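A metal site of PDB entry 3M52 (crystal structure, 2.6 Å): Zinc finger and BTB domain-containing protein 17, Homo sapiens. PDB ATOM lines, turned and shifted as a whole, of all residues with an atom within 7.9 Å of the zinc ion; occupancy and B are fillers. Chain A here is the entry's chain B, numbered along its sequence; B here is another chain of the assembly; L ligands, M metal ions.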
ATOM      1  N   PHE A   5     -25.142 -17.926  12.520  1.00  0.00           N
ATOM      2  CA  PHE A   5     -26.005 -16.859  12.003  1.00  0.00           C
ATOM      3  C   PHE A   5     -26.741 -17.330  10.728  1.00  0.00           C
ATOM      4  O   PHE A   5     -26.410 -16.867   9.634  1.00  0.00           O
ATOM      5  N   GLN A   7     -29.505 -16.798   9.186  1.00  0.00           N
ATOM      6  CA  GLN A   7     -30.122 -15.807   8.289  1.00  0.00           C
ATOM      7  C   GLN A   7     -29.170 -15.406   7.145  1.00  0.00           C
ATOM      8  O   GLN A   7     -29.613 -14.906   6.118  1.00  0.00           O
ATOM      9  CB  GLN A   7     -30.578 -14.569   9.072  1.00  0.00           C
ATOM     10  N   HIS A   8     -27.876 -15.623   7.342  1.00  0.00           N
ATOM     11  CA  HIS A   8     -26.865 -15.287   6.336  1.00  0.00           C
ATOM     12  C   HIS A   8     -26.997 -16.144   5.060  1.00  0.00           C
ATOM     13  O   HIS A   8     -26.650 -15.681   3.977  1.00  0.00           O
ATOM     14  CB  HIS A   8     -25.462 -15.324   6.943  1.00  0.00           C
ATOM     15  CG  HIS A   8     -24.371 -15.282   5.924  1.00  0.00           C
ATOM     16  ND1 HIS A   8     -24.009 -14.124   5.259  1.00  0.00           N
ATOM     17  CD2 HIS A   8     -23.555 -16.254   5.453  1.00  0.00           C
ATOM     18  CE1 HIS A   8     -23.019 -14.384   4.429  1.00  0.00           C
ATOM     19  NE2 HIS A   8     -22.726 -15.676   4.528  1.00  0.00           N
ATOM     20  N   SER A   9     -27.483 -17.376   5.201  1.00  0.00           N
ATOM     21  CA  SER A   9     -27.828 -18.238   4.052  1.00  0.00           C
ATOM     22  C   SER A   9     -28.819 -17.516   3.138  1.00  0.00           C
ATOM     23  O   SER A   9     -28.563 -17.333   1.937  1.00  0.00           O
ATOM     24  CB  SER A   9     -28.483 -19.545   4.510  1.00  0.00           C
ATOM     25  OG  SER A   9     -27.730 -20.210   5.501  1.00  0.00           O
ATOM     26  N   GLN A  10     -29.939 -17.087   3.725  1.00  0.00           N
ATOM     27  CA  GLN A  10     -30.989 -16.355   3.034  1.00  0.00           C
ATOM     28  C   GLN A  10     -30.443 -15.120   2.342  1.00  0.00           C
ATOM     29  O   GLN A  10     -30.958 -14.706   1.313  1.00  0.00           O
ATOM     30  CB  GLN A  10     -32.089 -15.931   4.003  1.00  0.00           C
ATOM     31  CG  GLN A  10     -32.819 -17.086   4.652  1.00  0.00           C
ATOM     32  CD  GLN A  10     -33.750 -16.618   5.744  1.00  0.00           C
ATOM     33  OE1 GLN A  10     -34.657 -15.805   5.504  1.00  0.00           O
ATOM     34  NE2 GLN A  10     -33.548 -17.129   6.952  1.00  0.00           N
ATOM     35  N   HIS A  11     -29.416 -14.521   2.943  1.00  0.00           N
ATOM     36  CA  HIS A  11     -28.749 -13.347   2.376  1.00  0.00           C
ATOM     37  C   HIS A  11     -27.948 -13.702   1.121  1.00  0.00           C
ATOM     38  O   HIS A  11     -27.970 -12.962   0.132  1.00  0.00           O
ATOM     39  CB  HIS A  11     -27.867 -12.691   3.456  1.00  0.00           C
ATOM     40  CG  HIS A  11     -26.903 -11.668   2.933  1.00  0.00           C
ATOM     41  ND1 HIS A  11     -25.603 -11.591   3.375  1.00  0.00           N
ATOM     42  CD2 HIS A  11     -27.052 -10.690   2.003  1.00  0.00           C
ATOM     43  CE1 HIS A  11     -24.978 -10.615   2.736  1.00  0.00           C
ATOM     44  NE2 HIS A  11     -25.838 -10.049   1.904  1.00  0.00           N
ATOM     45  N   VAL A  12     -27.270 -14.849   1.143  1.00  0.00           N
ATOM     46  CA  VAL A  12     -26.431 -15.282   0.022  1.00  0.00           C
ATOM     47  C   VAL A  12     -27.266 -15.631  -1.225  1.00  0.00           C
ATOM     48  O   VAL A  12     -26.995 -15.142  -2.325  1.00  0.00           O
ATOM     49  CB  VAL A  12     -25.484 -16.443   0.401  1.00  0.00           C
ATOM     50  CG1 VAL A  12     -24.587 -16.788  -0.766  1.00  0.00           C
ATOM     51  CG2 VAL A  12     -24.642 -16.071   1.605  1.00  0.00           C
ATOM     52  N   GLN A  15     -29.152 -12.600  -2.764  1.00  0.00           N
ATOM     53  CA  GLN A  15     -28.222 -11.813  -3.546  1.00  0.00           C
ATOM     54  C   GLN A  15     -27.783 -12.496  -4.830  1.00  0.00           C
ATOM     55  O   GLN A  15     -27.484 -11.842  -5.824  1.00  0.00           O
ATOM     56  CB  GLN A  15     -26.996 -11.447  -2.707  1.00  0.00           C
ATOM     57  CG  GLN A  15     -27.278 -10.396  -1.636  1.00  0.00           C
ATOM     58  CD  GLN A  15     -27.552  -9.030  -2.220  1.00  0.00           C
ATOM     59  OE1 GLN A  15     -26.876  -8.603  -3.154  1.00  0.00           O
ATOM     60  NE2 GLN A  15     -28.548  -8.348  -1.670  1.00  0.00           N
ATOM     61  N   ALA B  46     -22.051 -11.719  -3.434  1.00  0.00           N
ATOM     62  CA  ALA B  46     -23.320 -11.913  -2.737  1.00  0.00           C
ATOM     63  C   ALA B  46     -23.217 -11.472  -1.281  1.00  0.00           C
ATOM     64  O   ALA B  46     -24.208 -11.035  -0.683  1.00  0.00           O
ATOM     65  CB  ALA B  46     -23.758 -13.378  -2.816  1.00  0.00           C
ATOM     66  N   CYS B  47     -22.008 -11.580  -0.731  1.00  0.00           N
ATOM     67  CA  CYS B  47     -21.736 -11.275   0.673  1.00  0.00           C
ATOM     68  C   CYS B  47     -21.356  -9.825   0.908  1.00  0.00           C
ATOM     69  O   CYS B  47     -21.677  -9.268   1.962  1.00  0.00           O
ATOM     70  CB  CYS B  47     -20.621 -12.172   1.202  1.00  0.00           C
ATOM     71  SG  CYS B  47     -21.114 -13.884   1.430  1.00  0.00           S
ATOM     72  N   SER B  48     -20.700  -9.216  -0.070  1.00  0.00           N
ATOM     73  CA  SER B  48     -20.113  -7.899   0.131  1.00  0.00           C
ATOM     74  C   SER B  48     -20.178  -7.015  -1.101  1.00  0.00           C
ATOM     75  O   SER B  48     -19.794  -7.433  -2.191  1.00  0.00           O
ATOM     76  CB  SER B  48     -18.656  -8.042   0.589  1.00  0.00           C
ATOM     77  OG  SER B  48     -17.998  -6.779   0.635  1.00  0.00           O
ATOM     78  N   PHE B  78     -17.010 -17.239   7.481  1.00  0.00           N
ATOM     79  CA  PHE B  78     -18.413 -16.868   7.715  1.00  0.00           C
ATOM     80  C   PHE B  78     -19.229 -16.930   6.418  1.00  0.00           C
ATOM     81  O   PHE B  78     -20.312 -17.523   6.396  1.00  0.00           O
ATOM     82  CB  PHE B  78     -18.539 -15.462   8.329  1.00  0.00           C
ATOM     83  CG  PHE B  78     -19.971 -15.059   8.647  1.00  0.00           C
ATOM     84  CD1 PHE B  78     -20.748 -14.398   7.688  1.00  0.00           C
ATOM     85  CD2 PHE B  78     -20.527 -15.328   9.897  1.00  0.00           C
ATOM     86  CE1 PHE B  78     -22.052 -14.013   7.975  1.00  0.00           C
ATOM     87  CE2 PHE B  78     -21.843 -14.955  10.199  1.00  0.00           C
ATOM     88  CZ  PHE B  78     -22.614 -14.293   9.232  1.00  0.00           C
ATOM     89  N   MET B  79     -18.691 -16.314   5.363  1.00  0.00           N
ATOM     90  CA  MET B  79     -19.361 -16.236   4.069  1.00  0.00           C
ATOM     91  C   MET B  79     -19.950 -17.566   3.625  1.00  0.00           C
ATOM     92  O   MET B  79     -21.081 -17.617   3.127  1.00  0.00           O
ATOM     93  CB  MET B  79     -18.385 -15.747   3.006  1.00  0.00           C
ATOM     94  CG  MET B  79     -18.040 -14.279   3.090  1.00  0.00           C
ATOM     95  SD  MET B  79     -16.899 -13.812   1.783  1.00  0.00           S
ATOM     96  CE  MET B  79     -16.867 -12.043   1.969  1.00  0.00           C
ATOM     97  N   ALA B  82     -21.705 -19.380   7.612  1.00  0.00           N
ATOM     98  CA  ALA B  82     -22.598 -18.570   8.448  1.00  0.00           C
ATOM     99  C   ALA B  82     -22.266 -18.758   9.937  1.00  0.00           C
ATOM    100  O   ALA B  82     -23.100 -18.489  10.812  1.00  0.00           O
ATOM    101  CB  ALA B  82     -24.076 -18.881   8.145  1.00  0.00           C
ATOM    102  N   GLN B 102     -19.139  -4.090   4.272  1.00  0.00           N
ATOM    103  CA  GLN B 102     -20.587  -3.864   4.225  1.00  0.00           C
ATOM    104  C   GLN B 102     -21.363  -5.186   4.334  1.00  0.00           C
ATOM    105  O   GLN B 102     -22.316  -5.428   3.594  1.00  0.00           O
ATOM    106  CB  GLN B 102     -21.005  -3.056   2.977  1.00  0.00           C
ATOM    107  CG  GLN B 102     -20.673  -1.557   3.029  1.00  0.00           C
ATOM    108  CD  GLN B 102     -20.898  -0.869   1.699  1.00  0.00           C
ATOM    109  OE1 GLN B 102     -20.050  -0.904   0.800  1.00  0.00           O
ATOM    110  NE2 GLN B 102     -22.052  -0.212   1.553  1.00  0.00           N
ATOM    111  N   MET B 103     -20.912  -6.020   5.261  1.00  0.00           N
ATOM    112  CA  MET B 103     -21.571  -7.286   5.544  1.00  0.00           C
ATOM    113  C   MET B 103     -22.408  -7.155   6.819  1.00  0.00           C
ATOM    114  O   MET B 103     -21.871  -7.182   7.940  1.00  0.00           O
ATOM    115  CB  MET B 103     -20.526  -8.391   5.664  1.00  0.00           C
ATOM    116  CG  MET B 103     -19.689  -8.584   4.407  1.00  0.00           C
ATOM    117  SD  MET B 103     -18.331  -9.745   4.646  1.00  0.00           S
ATOM    118  CE  MET B 103     -19.225 -11.302   4.686  1.00  0.00           C
ATOM    119  N   GLN B 104     -23.715  -6.991   6.657  1.00  0.00           N
ATOM    120  CA  GLN B 104     -24.592  -6.621   7.779  1.00  0.00           C
ATOM    121  C   GLN B 104     -24.782  -7.733   8.824  1.00  0.00           C
ATOM    122  O   GLN B 104     -24.834  -7.438  10.027  1.00  0.00           O
ATOM    123  CB  GLN B 104     -25.944  -6.076   7.288  1.00  0.00           C
ATOM    124  CG  GLN B 104     -26.804  -5.380   8.363  1.00  0.00           C
ATOM    125  CD  GLN B 104     -26.166  -4.096   8.942  1.00  0.00           C
ATOM    126  OE1 GLN B 104     -25.377  -3.418   8.278  1.00  0.00           O
ATOM    127  NE2 GLN B 104     -26.530  -3.777  10.187  1.00  0.00           N
ATOM    128  N   ASP B 105     -24.874  -8.987   8.391  1.00  0.00           N
ATOM    129  CA  ASP B 105     -25.020 -10.108   9.329  1.00  0.00           C
ATOM    130  C   ASP B 105     -23.901 -10.125  10.368  1.00  0.00           C
ATOM    131  O   ASP B 105     -24.170 -10.357  11.539  1.00  0.00           O
ATOM    132  CB  ASP B 105     -25.097 -11.471   8.602  1.00  0.00           C
ATOM    133  CG  ASP B 105     -26.340 -11.614   7.727  1.00  0.00           C
ATOM    134  OD1 ASP B 105     -27.459 -11.308   8.185  1.00  0.00           O
ATOM    135  OD2 ASP B 105     -26.196 -12.077   6.574  1.00  0.00           O
ATOM    136  N   ILE B 106     -22.652  -9.881   9.940  1.00  0.00           N
ATOM    137  CA  ILE B 106     -21.508  -9.849  10.864  1.00  0.00           C
ATOM    138  C   ILE B 106     -21.492  -8.580  11.723  1.00  0.00           C
ATOM    139  O   ILE B 106     -21.229  -8.643  12.920  1.00  0.00           O
ATOM    140  CB  ILE B 106     -20.154  -9.968  10.129  1.00  0.00           C
ATOM    141  CG1 ILE B 106     -20.028 -11.318   9.433  1.00  0.00           C
ATOM    142  CG2 ILE B 106     -18.983  -9.798  11.129  1.00  0.00           C
ATOM    143  CD1 ILE B 106     -18.976 -11.335   8.351  1.00  0.00           C
HETATM  144  C1  LIG L   1     -23.103 -10.914   5.616  1.00  0.00           C
HETATM  145  O1  LIG L   1     -22.569 -11.397   4.596  1.00  0.00           O
HETATM  146  O2  LIG L   1     -24.172 -10.311   5.477  1.00  0.00           O
HETATM  147  C2  LIG L   1     -22.413 -11.013   6.935  1.00  0.00           C
HETATM  148 ZN    ZN M   1     -24.759 -12.185   5.194  1.00  0.00          ZN
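The zinc ion is bound by an oxygen (O2) of the ligand, the side-chain carboxylate of Asp 105 of chain B, a ring nitrogen (ND1) of His 8, a ring nitrogen (ND1) of His 11 and an oxygen (O1) of the ligand.
NE2 of His 8 is in hydrogen-bond range of O of Met 79 of chain B (2.9 Å).
A ring nitrogen (NE2) of His 11 is in hydrogen-bond range of the backbone carbonyl oxygen (O) of Ala 46 of chain B, 3.2 Å away.
Within 4 Å of the zinc ion: His 8, His 11 and Asp 105 of chain B.
The nearest printed residue that does not touch the zinc ion is Phe 78 of chain B (4.3 Å).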
